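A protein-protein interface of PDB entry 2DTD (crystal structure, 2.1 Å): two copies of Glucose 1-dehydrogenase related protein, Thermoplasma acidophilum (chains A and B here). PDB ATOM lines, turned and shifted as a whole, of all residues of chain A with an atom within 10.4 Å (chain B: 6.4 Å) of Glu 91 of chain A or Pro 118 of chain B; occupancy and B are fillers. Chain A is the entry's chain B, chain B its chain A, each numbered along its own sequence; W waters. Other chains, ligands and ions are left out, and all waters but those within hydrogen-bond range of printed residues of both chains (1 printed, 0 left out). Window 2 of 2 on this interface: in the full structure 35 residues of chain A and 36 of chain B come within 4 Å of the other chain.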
ATOM      1  N   TYR A  87      19.713   8.836 -17.163  1.00  0.00           N
ATOM      2  CA  TYR A  87      19.291   9.508 -15.944  1.00  0.00           C
ATOM      3  C   TYR A  87      20.046   9.137 -14.678  1.00  0.00           C
ATOM      4  O   TYR A  87      20.571   8.032 -14.547  1.00  0.00           O
ATOM      5  CB  TYR A  87      17.794   9.261 -15.744  1.00  0.00           C
ATOM      6  CG  TYR A  87      16.988   9.537 -16.997  1.00  0.00           C
ATOM      7  CD1 TYR A  87      16.611  10.835 -17.338  1.00  0.00           C
ATOM      8  CD2 TYR A  87      16.656   8.501 -17.874  1.00  0.00           C
ATOM      9  CE1 TYR A  87      15.922  11.099 -18.526  1.00  0.00           C
ATOM     10  CE2 TYR A  87      15.972   8.753 -19.061  1.00  0.00           C
ATOM     11  CZ  TYR A  87      15.610  10.052 -19.382  1.00  0.00           C
ATOM     12  OH  TYR A  87      14.949  10.298 -20.564  1.00  0.00           O
ATOM     13  N   GLY A  88      20.083  10.079 -13.745  1.00  0.00           N
ATOM     14  CA  GLY A  88      20.764   9.859 -12.487  1.00  0.00           C
ATOM     15  C   GLY A  88      21.202  11.156 -11.839  1.00  0.00           C
ATOM     16  O   GLY A  88      21.497  12.144 -12.521  1.00  0.00           O
ATOM     17  N   LYS A  89      21.226  11.162 -10.512  1.00  0.00           N
ATOM     18  CA  LYS A  89      21.655  12.337  -9.781  1.00  0.00           C
ATOM     19  C   LYS A  89      23.148  12.488  -9.977  1.00  0.00           C
ATOM     20  O   LYS A  89      23.839  11.525 -10.275  1.00  0.00           O
ATOM     21  CB  LYS A  89      21.319  12.201  -8.294  1.00  0.00           C
ATOM     22  CG  LYS A  89      19.896  12.637  -7.987  1.00  0.00           C
ATOM     23  CD  LYS A  89      19.558  12.556  -6.513  1.00  0.00           C
ATOM     24  CE  LYS A  89      18.261  13.295  -6.241  1.00  0.00           C
ATOM     25  NZ  LYS A  89      17.196  12.900  -7.206  1.00  0.00           N
ATOM     26  N   ILE A  90      23.634  13.712  -9.829  1.00  0.00           N
ATOM     27  CA  ILE A  90      25.047  13.998 -10.001  1.00  0.00           C
ATOM     28  C   ILE A  90      25.867  13.063  -9.107  1.00  0.00           C
ATOM     29  O   ILE A  90      27.035  12.774  -9.385  1.00  0.00           O
ATOM     30  CB  ILE A  90      25.330  15.490  -9.663  1.00  0.00           C
ATOM     31  CG1 ILE A  90      26.703  15.902 -10.180  1.00  0.00           C
ATOM     32  CG2 ILE A  90      25.257  15.721  -8.166  1.00  0.00           C
ATOM     33  CD1 ILE A  90      27.004  17.390  -9.973  1.00  0.00           C
ATOM     34  N   GLU A  91      25.223  12.563  -8.054  1.00  0.00           N
ATOM     35  CA  GLU A  91      25.862  11.669  -7.094  1.00  0.00           C
ATOM     36  C   GLU A  91      26.040  10.225  -7.537  1.00  0.00           C
ATOM     37  O   GLU A  91      27.078   9.621  -7.271  1.00  0.00           O
ATOM     38  CB  GLU A  91      25.081  11.658  -5.772  1.00  0.00           C
ATOM     39  CG  GLU A  91      25.104  12.965  -5.027  1.00  0.00           C
ATOM     40  CD  GLU A  91      26.481  13.590  -5.035  1.00  0.00           C
ATOM     41  OE1 GLU A  91      27.477  12.831  -4.956  1.00  0.00           O
ATOM     42  OE2 GLU A  91      26.568  14.837  -5.113  1.00  0.00           O
ATOM     43  N   SER A  92      25.026   9.669  -8.193  1.00  0.00           N
ATOM     44  CA  SER A  92      25.074   8.273  -8.617  1.00  0.00           C
ATOM     45  C   SER A  92      25.657   8.011 -10.007  1.00  0.00           C
ATOM     46  O   SER A  92      26.434   7.069 -10.182  1.00  0.00           O
ATOM     47  CB  SER A  92      23.672   7.658  -8.530  1.00  0.00           C
ATOM     48  OG  SER A  92      22.794   8.262  -9.465  1.00  0.00           O
ATOM     49  N   MET A  93      25.274   8.817 -10.995  1.00  0.00           N
ATOM     50  CA  MET A  93      25.793   8.621 -12.348  1.00  0.00           C
ATOM     51  C   MET A  93      27.310   8.699 -12.318  1.00  0.00           C
ATOM     52  O   MET A  93      27.874   9.603 -11.708  1.00  0.00           O
ATOM     53  CB  MET A  93      25.251   9.685 -13.311  1.00  0.00           C
ATOM     54  CG  MET A  93      25.752   9.500 -14.747  1.00  0.00           C
ATOM     55  SD  MET A  93      25.078  10.688 -15.949  1.00  0.00           S
ATOM     56  CE  MET A  93      23.534   9.886 -16.336  1.00  0.00           C
ATOM     57  N   SER A  94      27.969   7.748 -12.969  1.00  0.00           N
ATOM     58  CA  SER A  94      29.425   7.737 -13.008  1.00  0.00           C
ATOM     59  C   SER A  94      29.931   8.958 -13.765  1.00  0.00           C
ATOM     60  O   SER A  94      29.232   9.502 -14.624  1.00  0.00           O
ATOM     61  CB  SER A  94      29.938   6.483 -13.715  1.00  0.00           C
ATOM     62  OG  SER A  94      29.725   6.579 -15.112  1.00  0.00           O
ATOM     63  N   MET A  95      31.152   9.379 -13.451  1.00  0.00           N
ATOM     64  CA  MET A  95      31.736  10.523 -14.123  1.00  0.00           C
ATOM     65  C   MET A  95      31.943  10.234 -15.609  1.00  0.00           C
ATOM     66  O   MET A  95      31.827  11.131 -16.441  1.00  0.00           O
ATOM     67  CB  MET A  95      33.051  10.903 -13.462  1.00  0.00           C
ATOM     68  CG  MET A  95      32.859  11.428 -12.041  1.00  0.00           C
ATOM     69  SD  MET A  95      34.345  12.178 -11.416  1.00  0.00           S
ATOM     70  CE  MET A  95      35.487  10.749 -11.471  1.00  0.00           C
ATOM     71  N   GLY A  96      32.234   8.976 -15.930  1.00  0.00           N
ATOM     72  CA  GLY A  96      32.443   8.590 -17.314  1.00  0.00           C
ATOM     73  C   GLY A  96      31.177   8.765 -18.133  1.00  0.00           C
ATOM     74  O   GLY A  96      31.216   9.268 -19.255  1.00  0.00           O
ATOM     75  N   TRP A  98      28.674  10.733 -17.395  1.00  0.00           N
ATOM     76  CA  TRP A  98      28.318  12.146 -17.396  1.00  0.00           C
ATOM     77  C   TRP A  98      29.123  12.882 -18.477  1.00  0.00           C
ATOM     78  O   TRP A  98      28.562  13.693 -19.214  1.00  0.00           O
ATOM     79  CB  TRP A  98      28.588  12.751 -16.013  1.00  0.00           C
ATOM     80  CG  TRP A  98      27.789  13.994 -15.697  1.00  0.00           C
ATOM     81  CD1 TRP A  98      26.586  14.056 -15.036  1.00  0.00           C
ATOM     82  CD2 TRP A  98      28.140  15.346 -16.019  1.00  0.00           C
ATOM     83  NE1 TRP A  98      26.174  15.365 -14.928  1.00  0.00           N
ATOM     84  CE2 TRP A  98      27.108  16.178 -15.521  1.00  0.00           C
ATOM     85  CE3 TRP A  98      29.229  15.940 -16.681  1.00  0.00           C
ATOM     86  CZ2 TRP A  98      27.131  17.574 -15.660  1.00  0.00           C
ATOM     87  CZ3 TRP A  98      29.250  17.339 -16.819  1.00  0.00           C
ATOM     88  CH2 TRP A  98      28.206  18.131 -16.309  1.00  0.00           C
ATOM     89  N   ASN A 142      16.845  14.698 -12.485  1.00  0.00           N
ATOM     90  CA  ASN A 142      17.812  13.622 -12.684  1.00  0.00           C
ATOM     91  C   ASN A 142      18.368  13.556 -14.099  1.00  0.00           C
ATOM     92  O   ASN A 142      18.695  12.467 -14.589  1.00  0.00           O
ATOM     93  CB  ASN A 142      17.179  12.274 -12.326  1.00  0.00           C
ATOM     94  CG  ASN A 142      16.647  12.246 -10.910  1.00  0.00           C
ATOM     95  OD1 ASN A 142      17.309  12.707  -9.979  1.00  0.00           O
ATOM     96  ND2 ASN A 142      15.452  11.699 -10.736  1.00  0.00           N
ATOM     97  N   ALA A 143      18.482  14.717 -14.743  1.00  0.00           N
ATOM     98  CA  ALA A 143      18.990  14.783 -16.110  1.00  0.00           C
ATOM     99  C   ALA A 143      20.131  15.803 -16.225  1.00  0.00           C
ATOM    100  O   ALA A 143      20.305  16.465 -17.260  1.00  0.00           O
ATOM    101  CB  ALA A 143      17.844  15.138 -17.075  1.00  0.00           C
ATOM    102  N   SER A 144      20.908  15.896 -15.149  1.00  0.00           N
ATOM    103  CA  SER A 144      22.044  16.804 -15.021  1.00  0.00           C
ATOM    104  C   SER A 144      22.892  16.988 -16.286  1.00  0.00           C
ATOM    105  O   SER A 144      23.004  18.092 -16.825  1.00  0.00           O
ATOM    106  CB  SER A 144      22.947  16.312 -13.883  1.00  0.00           C
ATOM    107  OG  SER A 144      24.033  17.181 -13.696  1.00  0.00           O
ATOM    108  N   ALA A 145      23.507  15.901 -16.743  1.00  0.00           N
ATOM    109  CA  ALA A 145      24.357  15.942 -17.921  1.00  0.00           C
ATOM    110  C   ALA A 145      23.596  16.354 -19.185  1.00  0.00           C
ATOM    111  O   ALA A 145      24.090  17.150 -19.983  1.00  0.00           O
ATOM    112  CB  ALA A 145      25.012  14.577 -18.132  1.00  0.00           C
ATOM    113  N   SER B 113      30.803  20.223  -7.001  1.00  0.00           N
ATOM    114  CA  SER B 113      29.409  19.996  -6.602  1.00  0.00           C
ATOM    115  C   SER B 113      29.122  18.538  -6.279  1.00  0.00           C
ATOM    116  O   SER B 113      28.528  18.228  -5.253  1.00  0.00           O
ATOM    117  CB  SER B 113      28.446  20.451  -7.713  1.00  0.00           C
ATOM    118  OG  SER B 113      28.590  21.839  -7.964  1.00  0.00           O
ATOM    119  N   LYS B 114      29.539  17.647  -7.172  1.00  0.00           N
ATOM    120  CA  LYS B 114      29.328  16.215  -7.014  1.00  0.00           C
ATOM    121  C   LYS B 114      29.866  15.655  -5.684  1.00  0.00           C
ATOM    122  O   LYS B 114      29.227  14.814  -5.048  1.00  0.00           O
ATOM    123  CB  LYS B 114      29.993  15.469  -8.178  1.00  0.00           C
ATOM    124  CG  LYS B 114      29.732  13.981  -8.198  1.00  0.00           C
ATOM    125  CD  LYS B 114      30.507  13.294  -9.317  1.00  0.00           C
ATOM    126  CE  LYS B 114      30.866  11.870  -8.921  1.00  0.00           C
ATOM    127  NZ  LYS B 114      29.687  11.008  -8.637  1.00  0.00           N
ATOM    128  N   PHE B 115      31.033  16.124  -5.263  1.00  0.00           N
ATOM    129  CA  PHE B 115      31.623  15.617  -4.032  1.00  0.00           C
ATOM    130  C   PHE B 115      31.219  16.342  -2.759  1.00  0.00           C
ATOM    131  O   PHE B 115      31.246  15.755  -1.686  1.00  0.00           O
ATOM    132  CB  PHE B 115      33.144  15.574  -4.174  1.00  0.00           C
ATOM    133  CG  PHE B 115      33.600  14.664  -5.270  1.00  0.00           C
ATOM    134  CD1 PHE B 115      34.230  15.175  -6.405  1.00  0.00           C
ATOM    135  CD2 PHE B 115      33.308  13.302  -5.218  1.00  0.00           C
ATOM    136  CE1 PHE B 115      34.554  14.343  -7.481  1.00  0.00           C
ATOM    137  CE2 PHE B 115      33.626  12.460  -6.293  1.00  0.00           C
ATOM    138  CZ  PHE B 115      34.249  12.985  -7.425  1.00  0.00           C
ATOM    139  N   ALA B 116      30.831  17.607  -2.879  1.00  0.00           N
ATOM    140  CA  ALA B 116      30.424  18.376  -1.713  1.00  0.00           C
ATOM    141  C   ALA B 116      28.976  18.109  -1.311  1.00  0.00           C
ATOM    142  O   ALA B 116      28.650  18.094  -0.120  1.00  0.00           O
ATOM    143  CB  ALA B 116      30.614  19.870  -1.978  1.00  0.00           C
ATOM    144  N   ILE B 117      28.111  17.892  -2.299  1.00  0.00           N
ATOM    145  CA  ILE B 117      26.694  17.684  -2.024  1.00  0.00           C
ATOM    146  C   ILE B 117      26.363  16.627  -0.965  1.00  0.00           C
ATOM    147  O   ILE B 117      25.612  16.909  -0.027  1.00  0.00           O
ATOM    148  CB  ILE B 117      25.913  17.422  -3.340  1.00  0.00           C
ATOM    149  CG1 ILE B 117      25.836  18.727  -4.151  1.00  0.00           C
ATOM    150  CG2 ILE B 117      24.521  16.907  -3.036  1.00  0.00           C
ATOM    151  CD1 ILE B 117      25.267  18.584  -5.582  1.00  0.00           C
ATOM    152  N   PRO B 118      26.914  15.406  -1.090  1.00  0.00           N
ATOM    153  CA  PRO B 118      26.625  14.367  -0.094  1.00  0.00           C
ATOM    154  C   PRO B 118      26.857  14.854   1.340  1.00  0.00           C
ATOM    155  O   PRO B 118      26.112  14.499   2.250  1.00  0.00           O
ATOM    156  CB  PRO B 118      27.580  13.243  -0.485  1.00  0.00           C
ATOM    157  CG  PRO B 118      27.624  13.379  -1.995  1.00  0.00           C
ATOM    158  CD  PRO B 118      27.765  14.875  -2.173  1.00  0.00           C
ATOM    159  N   TYR B 119      27.891  15.670   1.529  1.00  0.00           N
ATOM    160  CA  TYR B 119      28.204  16.216   2.843  1.00  0.00           C
ATOM    161  C   TYR B 119      27.271  17.372   3.182  1.00  0.00           C
ATOM    162  O   TYR B 119      26.779  17.482   4.314  1.00  0.00           O
ATOM    163  CB  TYR B 119      29.642  16.729   2.885  1.00  0.00           C
ATOM    164  CG  TYR B 119      30.701  15.657   2.759  1.00  0.00           C
ATOM    165  CD1 TYR B 119      31.633  15.697   1.724  1.00  0.00           C
ATOM    166  CD2 TYR B 119      30.810  14.637   3.713  1.00  0.00           C
ATOM    167  CE1 TYR B 119      32.660  14.752   1.640  1.00  0.00           C
ATOM    168  CE2 TYR B 119      31.833  13.686   3.642  1.00  0.00           C
ATOM    169  CZ  TYR B 119      32.757  13.755   2.607  1.00  0.00           C
ATOM    170  OH  TYR B 119      33.799  12.863   2.557  1.00  0.00           O
ATOM    171  N   MET B 120      27.035  18.231   2.192  1.00  0.00           N
ATOM    172  CA  MET B 120      26.182  19.392   2.372  1.00  0.00           C
ATOM    173  C   MET B 120      24.766  19.060   2.830  1.00  0.00           C
ATOM    174  O   MET B 120      24.211  19.752   3.685  1.00  0.00           O
ATOM    175  CB  MET B 120      26.154  20.213   1.078  1.00  0.00           C
ATOM    176  CG  MET B 120      27.487  20.888   0.795  1.00  0.00           C
ATOM    177  SD  MET B 120      27.548  21.839  -0.737  1.00  0.00           S
ATOM    178  CE  MET B 120      26.676  23.300  -0.257  1.00  0.00           C
ATOM    179  N   ILE B 121      24.176  18.007   2.276  1.00  0.00           N
ATOM    180  CA  ILE B 121      22.833  17.649   2.685  1.00  0.00           C
ATOM    181  C   ILE B 121      22.800  17.131   4.125  1.00  0.00           C
ATOM    182  O   ILE B 121      21.743  16.781   4.638  1.00  0.00           O
ATOM    183  CB  ILE B 121      22.188  16.603   1.746  1.00  0.00           C
ATOM    184  CG1 ILE B 121      23.066  15.362   1.649  1.00  0.00           C
ATOM    185  CG2 ILE B 121      21.945  17.218   0.360  1.00  0.00           C
ATOM    186  CD1 ILE B 121      22.454  14.270   0.772  1.00  0.00           C
ATOM    187  N   ARG B 122      23.958  17.072   4.777  1.00  0.00           N
ATOM    188  CA  ARG B 122      23.993  16.633   6.166  1.00  0.00           C
ATOM    189  C   ARG B 122      23.923  17.842   7.087  1.00  0.00           C
ATOM    190  O   ARG B 122      23.925  17.694   8.308  1.00  0.00           O
ATOM    191  CB  ARG B 122      25.258  15.835   6.471  1.00  0.00           C
ATOM    192  CG  ARG B 122      25.328  14.486   5.793  1.00  0.00           C
ATOM    193  CD  ARG B 122      26.611  13.783   6.193  1.00  0.00           C
ATOM    194  NE  ARG B 122      27.049  12.837   5.178  1.00  0.00           N
ATOM    195  CZ  ARG B 122      28.157  12.108   5.268  1.00  0.00           C
ATOM    196  NH1 ARG B 122      28.935  12.219   6.340  1.00  0.00           N
ATOM    197  NH2 ARG B 122      28.492  11.286   4.277  1.00  0.00           N
ATOM    198  N   TYR B 164      17.910  18.515  -5.947  1.00  0.00           N
ATOM    199  CA  TYR B 164      18.004  18.493  -4.495  1.00  0.00           C
ATOM    200  C   TYR B 164      17.064  19.388  -3.684  1.00  0.00           C
ATOM    201  O   TYR B 164      17.167  19.430  -2.456  1.00  0.00           O
ATOM    202  CB  TYR B 164      19.458  18.752  -4.068  1.00  0.00           C
ATOM    203  CG  TYR B 164      20.417  17.695  -4.578  1.00  0.00           C
ATOM    204  CD1 TYR B 164      21.126  17.884  -5.767  1.00  0.00           C
ATOM    205  CD2 TYR B 164      20.554  16.473  -3.917  1.00  0.00           C
ATOM    206  CE1 TYR B 164      21.940  16.886  -6.288  1.00  0.00           C
ATOM    207  CE2 TYR B 164      21.365  15.463  -4.431  1.00  0.00           C
ATOM    208  CZ  TYR B 164      22.053  15.678  -5.620  1.00  0.00           C
ATOM    209  OH  TYR B 164      22.832  14.680  -6.152  1.00  0.00           O
HETATM  210  O   HOH W   1      29.660  11.973  -5.942  1.00  0.00           O
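No position is printed for both chains. Of the 11 pairs that touch across the chains among the printed residues, none has its exchanged pair printed and touching as well.
NZ of Lys 114 of chain B is in hydrogen-bond range of O of Glu 91 of chain A (3.3 Å). NZ of Lys 114 of chain B sits close to O of Ile 90 of chain A (3.3 Å).
Of chain B, only Ser 113 (3.9 Å), Lys 114 (2.6 Å), Ile 117 (3.2 Å), Pro 118 (3.0 Å) and Tyr 164 (3.1 Å) come within 4 Å of Glu 91 of chain A. Of chain A, only Glu 91 (3.0 Å) comes within 4 Å of Pro 118 of chain B. Lys 114 of chain B touches just these residues of chain A: Ile 90 (3.2 Å), Glu 91 (2.6 Å), Met 93 (3.8 Å) and Met 95 (3.7 Å). No residue of chain A comes within 4 Å of Ala 116 of chain B. Printed residues of chain A within 4 Å of Ile 117 of chain B: Ile 90 and Glu 91. No residue of chain A comes within 4 Å of Ile 121 of chain B. Printed residues of chain B within 4 Å of Met 95 of chain A: Lys 114 (3.7 Å). Of the printed residues of chain B, Lys 89 of chain A touches Tyr 164. Of the printed residues of chain B, Ile 90 of chain A touches Lys 114, Ile 117 and Tyr 164. The nearest printed residue of chain B that does not touch Met 95 of chain A is Phe 115 of chain B (4.1 Å).
Hydrophobic or aromatic side chains of chain B within 4 Å of the printed part of chain A: Ile 117, Pro 118 and Tyr 164. Of the 15 printed residues of chain A, 5 touch a printed residue of chain B. Printed residues of chain A that touch a printed residue of chain B: Lys 89, Ile 90, Glu 91, Met 93 and Met 95. Hydrophobic or aromatic side chains of chain A within 4 Å of the printed part of chain B: Ile 90 and Met 95.
Water W1 bridges OE1 of Glu 91 of chain A (2.5 Å) and NZ of Lys 114 of chain B (2.9 Å).
The side-chain amino group (NZ) of Lys 89 of chain A sits at hydrogen-bond distance from the side-chain amide oxygen (OD1) of Asn 142 of chain A. The side-chain hydroxyl (OG) of Ser 92 of chain A is in hydrogen-bond range of the backbone NH (N) of Lys 89 of chain A, at 3.5 Å. The backbone carbonyl oxygen (O) of Pro 118 of chain B sits at hydrogen-bond distance from the guanidinium group (NE) of Arg 122 of chain B (3.5 Å).
Among the printed residues, pairs that only touch across the chains: Lys 89 of chain A with Tyr 164 of chain B (3.6 Å), Ile 90 of chain A with Ile 117 of chain B (3.9 Å), Ile 90 of chain A with Tyr 164 of chain B (3.3 Å), Glu 91 of chain A with Ser 113 of chain B (3.9 Å), Glu 91 of chain A with Ile 117 of chain B (3.2 Å), Glu 91 of chain A with Pro 118 of chain B (3.0 Å), Glu 91 of chain A with Tyr 164 of chain B (3.1 Å), Met 93 of chain A with Lys 114 of chain B (3.8 Å) and Met 95 of chain A with Lys 114 of chain B (3.7 Å).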
